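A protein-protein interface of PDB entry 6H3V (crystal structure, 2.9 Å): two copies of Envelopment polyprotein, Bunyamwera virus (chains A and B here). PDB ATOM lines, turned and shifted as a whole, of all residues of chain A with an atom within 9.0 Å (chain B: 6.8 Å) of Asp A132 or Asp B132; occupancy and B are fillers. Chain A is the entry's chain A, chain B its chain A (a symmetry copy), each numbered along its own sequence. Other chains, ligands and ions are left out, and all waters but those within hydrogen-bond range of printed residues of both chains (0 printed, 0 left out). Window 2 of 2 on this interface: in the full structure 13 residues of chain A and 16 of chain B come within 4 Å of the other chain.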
ATOM      1  N   LYS A 110      16.500   3.720  12.524  1.00  0.00           N
ATOM      2  CA  LYS A 110      16.877   2.585  11.681  1.00  0.00           C
ATOM      3  C   LYS A 110      17.231   1.365  12.509  1.00  0.00           C
ATOM      4  O   LYS A 110      17.455   0.290  11.939  1.00  0.00           O
ATOM      5  CB  LYS A 110      18.046   2.936  10.728  1.00  0.00           C
ATOM      6  CG  LYS A 110      17.742   4.038   9.674  1.00  0.00           C
ATOM      7  CD  LYS A 110      16.691   3.630   8.627  1.00  0.00           C
ATOM      8  CE  LYS A 110      17.269   3.589   7.216  1.00  0.00           C
ATOM      9  NZ  LYS A 110      16.474   2.741   6.278  1.00  0.00           N
ATOM     10  N   PRO A 124       2.903   0.022   3.116  1.00  0.00           N
ATOM     11  CA  PRO A 124       3.999   0.700   2.403  1.00  0.00           C
ATOM     12  C   PRO A 124       4.973   1.426   3.307  1.00  0.00           C
ATOM     13  O   PRO A 124       6.151   1.527   2.951  1.00  0.00           O
ATOM     14  CB  PRO A 124       3.258   1.668   1.472  1.00  0.00           C
ATOM     15  CG  PRO A 124       1.948   0.999   1.229  1.00  0.00           C
ATOM     16  CD  PRO A 124       1.588   0.367   2.552  1.00  0.00           C
ATOM     17  N   PHE A 125       4.533   1.938   4.459  1.00  0.00           N
ATOM     18  CA  PHE A 125       5.485   2.539   5.392  1.00  0.00           C
ATOM     19  C   PHE A 125       6.587   1.546   5.752  1.00  0.00           C
ATOM     20  O   PHE A 125       7.769   1.781   5.474  1.00  0.00           O
ATOM     21  CB  PHE A 125       4.777   3.045   6.648  1.00  0.00           C
ATOM     22  CG  PHE A 125       5.709   3.697   7.641  1.00  0.00           C
ATOM     23  CD1 PHE A 125       6.457   4.812   7.284  1.00  0.00           C
ATOM     24  CD2 PHE A 125       5.839   3.195   8.937  1.00  0.00           C
ATOM     25  CE1 PHE A 125       7.315   5.417   8.202  1.00  0.00           C
ATOM     26  CE2 PHE A 125       6.698   3.790   9.863  1.00  0.00           C
ATOM     27  CZ  PHE A 125       7.432   4.903   9.499  1.00  0.00           C
ATOM     28  N   CYS A 126       6.208   0.418   6.362  1.00  0.00           N
ATOM     29  CA  CYS A 126       7.185  -0.588   6.765  1.00  0.00           C
ATOM     30  C   CYS A 126       8.030  -1.067   5.584  1.00  0.00           C
ATOM     31  O   CYS A 126       9.262  -0.933   5.592  1.00  0.00           O
ATOM     32  CB  CYS A 126       6.464  -1.764   7.423  1.00  0.00           C
ATOM     33  SG  CYS A 126       5.543  -1.315   8.903  1.00  0.00           S
ATOM     34  N   ALA A 127       7.382  -1.612   4.547  1.00  0.00           N
ATOM     35  CA  ALA A 127       8.109  -2.323   3.498  1.00  0.00           C
ATOM     36  C   ALA A 127       8.801  -1.401   2.502  1.00  0.00           C
ATOM     37  O   ALA A 127       9.692  -1.855   1.776  1.00  0.00           O
ATOM     38  CB  ALA A 127       7.167  -3.264   2.749  1.00  0.00           C
ATOM     39  N   GLN A 128       8.428  -0.126   2.453  1.00  0.00           N
ATOM     40  CA  GLN A 128       9.021   0.821   1.518  1.00  0.00           C
ATOM     41  C   GLN A 128       9.839   1.892   2.232  1.00  0.00           C
ATOM     42  O   GLN A 128      10.993   2.116   1.864  1.00  0.00           O
ATOM     43  CB  GLN A 128       7.942   1.427   0.605  1.00  0.00           C
ATOM     44  CG  GLN A 128       7.160   0.347  -0.171  1.00  0.00           C
ATOM     45  CD  GLN A 128       6.246   0.912  -1.245  1.00  0.00           C
ATOM     46  OE1 GLN A 128       6.339   2.087  -1.587  1.00  0.00           O
ATOM     47  NE2 GLN A 128       5.359   0.073  -1.784  1.00  0.00           N
ATOM     48  N   CYS A 129       9.256   2.626   3.187  1.00  0.00           N
ATOM     49  CA  CYS A 129       9.960   3.749   3.813  1.00  0.00           C
ATOM     50  C   CYS A 129      10.986   3.329   4.885  1.00  0.00           C
ATOM     51  O   CYS A 129      12.147   3.749   4.831  1.00  0.00           O
ATOM     52  CB  CYS A 129       8.933   4.730   4.389  1.00  0.00           C
ATOM     53  SG  CYS A 129       9.579   6.373   4.857  1.00  0.00           S
ATOM     54  N   ILE A 130      10.592   2.515   5.875  1.00  0.00           N
ATOM     55  CA  ILE A 130      11.506   2.215   6.988  1.00  0.00           C
ATOM     56  C   ILE A 130      12.659   1.338   6.515  1.00  0.00           C
ATOM     57  O   ILE A 130      13.828   1.570   6.858  1.00  0.00           O
ATOM     58  CB  ILE A 130      10.749   1.553   8.158  1.00  0.00           C
ATOM     59  CG1 ILE A 130       9.947   2.590   8.955  1.00  0.00           C
ATOM     60  CG2 ILE A 130      11.711   0.797   9.070  1.00  0.00           C
ATOM     61  CD1 ILE A 130      10.786   3.675   9.614  1.00  0.00           C
ATOM     62  N   ALA A 131      12.349   0.325   5.715  1.00  0.00           N
ATOM     63  CA  ALA A 131      13.361  -0.531   5.120  1.00  0.00           C
ATOM     64  C   ALA A 131      14.101   0.159   3.979  1.00  0.00           C
ATOM     65  O   ALA A 131      15.273   0.532   4.124  1.00  0.00           O
ATOM     66  CB  ALA A 131      12.703  -1.806   4.609  1.00  0.00           C
ATOM     67  N   ASP A 132      13.411   0.360   2.848  1.00  0.00           N
ATOM     68  CA  ASP A 132      14.072   0.766   1.610  1.00  0.00           C
ATOM     69  C   ASP A 132      14.521   2.227   1.623  1.00  0.00           C
ATOM     70  O   ASP A 132      15.331   2.618   0.777  1.00  0.00           O
ATOM     71  CB  ASP A 132      13.152   0.501   0.409  1.00  0.00           C
ATOM     72  CG  ASP A 132      12.857  -0.990   0.200  1.00  0.00           C
ATOM     73  OD1 ASP A 132      13.297  -1.822   1.028  1.00  0.00           O
ATOM     74  OD2 ASP A 132      12.177  -1.330  -0.792  1.00  0.00           O
ATOM     75  N   ASN A 133      14.013   3.039   2.553  1.00  0.00           N
ATOM     76  CA  ASN A 133      14.394   4.434   2.790  1.00  0.00           C
ATOM     77  C   ASN A 133      13.955   5.361   1.650  1.00  0.00           C
ATOM     78  O   ASN A 133      14.208   6.576   1.722  1.00  0.00           O
ATOM     79  CB  ASN A 133      15.898   4.566   3.130  1.00  0.00           C
ATOM     80  CG  ASN A 133      16.739   5.234   2.034  1.00  0.00           C
ATOM     81  OD1 ASN A 133      16.596   4.958   0.843  1.00  0.00           O
ATOM     82  ND2 ASN A 133      17.651   6.106   2.456  1.00  0.00           N
ATOM     83  N   SER A 134      13.298   4.834   0.609  1.00  0.00           N
ATOM     84  CA  SER A 134      12.762   5.631  -0.491  1.00  0.00           C
ATOM     85  C   SER A 134      11.892   6.794  -0.014  1.00  0.00           C
ATOM     86  O   SER A 134      12.313   7.953  -0.075  1.00  0.00           O
ATOM     87  CB  SER A 134      11.948   4.730  -1.426  1.00  0.00           C
ATOM     88  OG  SER A 134      10.869   4.116  -0.733  1.00  0.00           O
ATOM     89  N   CYS A 135      10.677   6.487   0.455  1.00  0.00           N
ATOM     90  CA  CYS A 135       9.713   7.436   1.032  1.00  0.00           C
ATOM     91  C   CYS A 135       9.326   8.578   0.094  1.00  0.00           C
ATOM     92  O   CYS A 135       8.799   9.598   0.558  1.00  0.00           O
ATOM     93  CB  CYS A 135      10.221   8.036   2.344  1.00  0.00           C
ATOM     94  SG  CYS A 135      10.988   6.864   3.451  1.00  0.00           S
ATOM     95  N   ALA A 136       9.528   8.431  -1.220  1.00  0.00           N
ATOM     96  CA  ALA A 136       9.084   9.461  -2.150  1.00  0.00           C
ATOM     97  C   ALA A 136       7.577   9.429  -2.345  1.00  0.00           C
ATOM     98  O   ALA A 136       7.001  10.420  -2.807  1.00  0.00           O
ATOM     99  CB  ALA A 136       9.791   9.307  -3.499  1.00  0.00           C
ATOM    100  N   LEU A 208      12.693  10.264   4.783  1.00  0.00           N
ATOM    101  CA  LEU A 208      12.566   9.518   6.032  1.00  0.00           C
ATOM    102  C   LEU A 208      11.787  10.322   7.066  1.00  0.00           C
ATOM    103  O   LEU A 208      10.856   9.814   7.704  1.00  0.00           O
ATOM    104  CB  LEU A 208      13.951   9.166   6.566  1.00  0.00           C
ATOM    105  CG  LEU A 208      13.990   7.957   7.490  1.00  0.00           C
ATOM    106  CD1 LEU A 208      13.491   6.766   6.701  1.00  0.00           C
ATOM    107  CD2 LEU A 208      15.398   7.717   8.005  1.00  0.00           C
ATOM    108  N   LYS B 110      24.638   3.873   6.814  1.00  0.00           N
ATOM    109  CA  LYS B 110      23.273   3.354   6.897  1.00  0.00           C
ATOM    110  C   LYS B 110      22.349   4.320   7.613  1.00  0.00           C
ATOM    111  O   LYS B 110      21.137   4.077   7.658  1.00  0.00           O
ATOM    112  CB  LYS B 110      23.224   1.965   7.583  1.00  0.00           C
ATOM    113  CG  LYS B 110      23.962   0.821   6.832  1.00  0.00           C
ATOM    114  CD  LYS B 110      23.327   0.448   5.482  1.00  0.00           C
ATOM    115  CE  LYS B 110      22.807  -0.986   5.468  1.00  0.00           C
ATOM    116  NZ  LYS B 110      21.769  -1.227   4.420  1.00  0.00           N
ATOM    117  N   CYS B 117      19.019   9.931  -3.291  1.00  0.00           N
ATOM    118  CA  CYS B 117      18.188   8.777  -2.956  1.00  0.00           C
ATOM    119  C   CYS B 117      16.806   9.173  -2.487  1.00  0.00           C
ATOM    120  O   CYS B 117      15.881   8.358  -2.556  1.00  0.00           O
ATOM    121  CB  CYS B 117      18.865   7.946  -1.870  1.00  0.00           C
ATOM    122  SG  CYS B 117      20.261   7.081  -2.544  1.00  0.00           S
ATOM    123  N   ALA B 121      14.259   7.726  -5.983  1.00  0.00           N
ATOM    124  CA  ALA B 121      14.760   6.503  -5.362  1.00  0.00           C
ATOM    125  C   ALA B 121      14.740   5.307  -6.303  1.00  0.00           C
ATOM    126  O   ALA B 121      15.036   4.187  -5.868  1.00  0.00           O
ATOM    127  CB  ALA B 121      13.946   6.177  -4.103  1.00  0.00           C
ATOM    128  N   PHE B 125      21.319   2.049  -7.225  1.00  0.00           N
ATOM    129  CA  PHE B 125      22.108   2.303  -6.020  1.00  0.00           C
ATOM    130  C   PHE B 125      21.199   2.503  -4.811  1.00  0.00           C
ATOM    131  O   PHE B 125      21.249   1.732  -3.845  1.00  0.00           O
ATOM    132  CB  PHE B 125      23.031   3.506  -6.213  1.00  0.00           C
ATOM    133  CG  PHE B 125      23.889   3.803  -5.006  1.00  0.00           C
ATOM    134  CD1 PHE B 125      24.780   2.854  -4.520  1.00  0.00           C
ATOM    135  CD2 PHE B 125      23.808   5.035  -4.356  1.00  0.00           C
ATOM    136  CE1 PHE B 125      25.576   3.129  -3.408  1.00  0.00           C
ATOM    137  CE2 PHE B 125      24.597   5.320  -3.240  1.00  0.00           C
ATOM    138  CZ  PHE B 125      25.484   4.371  -2.768  1.00  0.00           C
ATOM    139  N   CYS B 126      20.348   3.533  -4.859  1.00  0.00           N
ATOM    140  CA  CYS B 126      19.448   3.823  -3.748  1.00  0.00           C
ATOM    141  C   CYS B 126      18.565   2.623  -3.402  1.00  0.00           C
ATOM    142  O   CYS B 126      18.604   2.114  -2.273  1.00  0.00           O
ATOM    143  CB  CYS B 126      18.591   5.042  -4.089  1.00  0.00           C
ATOM    144  SG  CYS B 126      19.546   6.539  -4.387  1.00  0.00           S
ATOM    145  N   ALA B 127      17.774   2.144  -4.370  1.00  0.00           N
ATOM    146  CA  ALA B 127      16.720   1.179  -4.069  1.00  0.00           C
ATOM    147  C   ALA B 127      17.233  -0.242  -3.871  1.00  0.00           C
ATOM    148  O   ALA B 127      16.511  -1.072  -3.307  1.00  0.00           O
ATOM    149  CB  ALA B 127      15.664   1.188  -5.173  1.00  0.00           C
ATOM    150  N   GLN B 128      18.452  -0.542  -4.305  1.00  0.00           N
ATOM    151  CA  GLN B 128      19.016  -1.879  -4.175  1.00  0.00           C
ATOM    152  C   GLN B 128      20.193  -1.913  -3.206  1.00  0.00           C
ATOM    153  O   GLN B 128      20.206  -2.747  -2.300  1.00  0.00           O
ATOM    154  CB  GLN B 128      19.385  -2.446  -5.556  1.00  0.00           C
ATOM    155  CG  GLN B 128      18.177  -2.479  -6.516  1.00  0.00           C
ATOM    156  CD  GLN B 128      18.446  -3.236  -7.805  1.00  0.00           C
ATOM    157  OE1 GLN B 128      19.447  -3.939  -7.920  1.00  0.00           O
ATOM    158  NE2 GLN B 128      17.549  -3.097  -8.783  1.00  0.00           N
ATOM    159  N   CYS B 129      21.228  -1.090  -3.413  1.00  0.00           N
ATOM    160  CA  CYS B 129      22.436  -1.172  -2.585  1.00  0.00           C
ATOM    161  C   CYS B 129      22.295  -0.505  -1.202  1.00  0.00           C
ATOM    162  O   CYS B 129      22.591  -1.132  -0.178  1.00  0.00           O
ATOM    163  CB  CYS B 129      23.619  -0.585  -3.362  1.00  0.00           C
ATOM    164  SG  CYS B 129      25.274  -0.946  -2.677  1.00  0.00           S
ATOM    165  N   ILE B 130      21.861   0.761  -1.133  1.00  0.00           N
ATOM    166  CA  ILE B 130      21.856   1.469   0.156  1.00  0.00           C
ATOM    167  C   ILE B 130      20.794   0.889   1.082  1.00  0.00           C
ATOM    168  O   ILE B 130      21.035   0.665   2.277  1.00  0.00           O
ATOM    169  CB  ILE B 130      21.648   2.984  -0.049  1.00  0.00           C
ATOM    170  CG1 ILE B 130      22.938   3.658  -0.536  1.00  0.00           C
ATOM    171  CG2 ILE B 130      21.146   3.643   1.232  1.00  0.00           C
ATOM    172  CD1 ILE B 130      24.110   3.565   0.431  1.00  0.00           C
ATOM    173  N   ALA B 131      19.608   0.635   0.543  1.00  0.00           N
ATOM    174  CA  ALA B 131      18.537  -0.001   1.291  1.00  0.00           C
ATOM    175  C   ALA B 131      18.781  -1.494   1.490  1.00  0.00           C
ATOM    176  O   ALA B 131      19.094  -1.937   2.604  1.00  0.00           O
ATOM    177  CB  ALA B 131      17.218   0.210   0.560  1.00  0.00           C
ATOM    178  N   ASP B 132      18.671  -2.273   0.405  1.00  0.00           N
ATOM    179  CA  ASP B 132      18.621  -3.730   0.510  1.00  0.00           C
ATOM    180  C   ASP B 132      19.977  -4.350   0.845  1.00  0.00           C
ATOM    181  O   ASP B 132      20.025  -5.519   1.240  1.00  0.00           O
ATOM    182  CB  ASP B 132      18.064  -4.332  -0.788  1.00  0.00           C
ATOM    183  CG  ASP B 132      16.608  -3.931  -1.056  1.00  0.00           C
ATOM    184  OD1 ASP B 132      16.045  -3.121  -0.284  1.00  0.00           O
ATOM    185  OD2 ASP B 132      16.027  -4.423  -2.048  1.00  0.00           O
ATOM    186  N   ASN B 133      21.073  -3.604   0.694  1.00  0.00           N
ATOM    187  CA  ASN B 133      22.441  -3.984   1.058  1.00  0.00           C
ATOM    188  C   ASN B 133      22.996  -5.095   0.159  1.00  0.00           C
ATOM    189  O   ASN B 133      24.152  -5.513   0.351  1.00  0.00           O
ATOM    190  CB  ASN B 133      22.561  -4.310   2.566  1.00  0.00           C
ATOM    191  CG  ASN B 133      22.791  -5.795   2.877  1.00  0.00           C
ATOM    192  OD1 ASN B 133      22.169  -6.686   2.299  1.00  0.00           O
ATOM    193  ND2 ASN B 133      23.681  -6.055   3.830  1.00  0.00           N
ATOM    194  N   SER B 134      22.221  -5.579  -0.819  1.00  0.00           N
ATOM    195  CA  SER B 134      22.673  -6.578  -1.785  1.00  0.00           C
ATOM    196  C   SER B 134      23.987  -6.195  -2.465  1.00  0.00           C
ATOM    197  O   SER B 134      25.036  -6.775  -2.167  1.00  0.00           O
ATOM    198  CB  SER B 134      21.588  -6.791  -2.846  1.00  0.00           C
ATOM    199  OG  SER B 134      21.301  -5.582  -3.534  1.00  0.00           O
ATOM    200  N   CYS B 135      23.931  -5.224  -3.383  1.00  0.00           N
ATOM    201  CA  CYS B 135      25.081  -4.650  -4.100  1.00  0.00           C
ATOM    202  C   CYS B 135      25.900  -5.674  -4.883  1.00  0.00           C
ATOM    203  O   CYS B 135      27.049  -5.389  -5.246  1.00  0.00           O
ATOM    204  CB  CYS B 135      26.022  -3.896  -3.157  1.00  0.00           C
ATOM    205  SG  CYS B 135      25.198  -2.863  -1.955  1.00  0.00           S
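OD1 of Asp B132 lies close to OD1 of Asp A132, 3.3 Å away.
Lys B110 touches its own counterpart, Lys A110. Asp A132 touches Ala B131, but with the chains exchanged Ala A131 does not touch Asp B132 (5.7 Å). Asp B132 touches its own counterpart, Asp A132.
Asp A132 touches just these residues of chain B: Ala B131 (3.1 Å) and Asp B132 (3.3 Å). Of chain A, only Asp A132 (3.3 Å) comes within 4 Å of Asp B132. No residue of chain A comes within 4 Å of Asn B133. Printed residues of chain B within 4 Å of Ser A134: Ala B121 (3.6 Å). Of the printed residues of chain B, Lys A110 touches Lys B110 (3.9 Å). Printed residues of chain A within 4 Å of Ala B121: Ser A134. Of the printed residues of chain A, Lys B110 touches Lys A110 (3.9 Å).
NZ of Lys A110 lies within hydrogen-bond range of O of Ile A130, at 3.0 Å. The backbone carbonyl oxygen (O) of Gln A128 lies within hydrogen-bond range of the side-chain hydroxyl (OG) of Ser A134 (3.3 Å). The side-chain amino group of Lys B110 lies within hydrogen-bond range of the backbone carbonyl oxygen of Ile B130, at 3.0 Å. The backbone carbonyl oxygen (O) of Ala B131 is in hydrogen-bond range of the side-chain amino group (NZ) of Lys B110, 3.3 Å away. The backbone NH (N) of Ala B131 lies within hydrogen-bond range of the backbone carbonyl oxygen (O) of Cys B126 (3.3 Å). SG of Cys A135 is disulfide-bonded to SG of Cys A129.
Of the 15 printed residues of chain A, 3 touch a printed residue of chain B. Among the printed residues, no Asp or Glu carboxylate lies within 4 Å of a Lys or Arg side-chain nitrogen of the other chain.
Lys A110 touches Lys B110. Asp A132 touches Ala B131 (O to CB, 3.1 Å). Ala B121 touches Ser A134.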
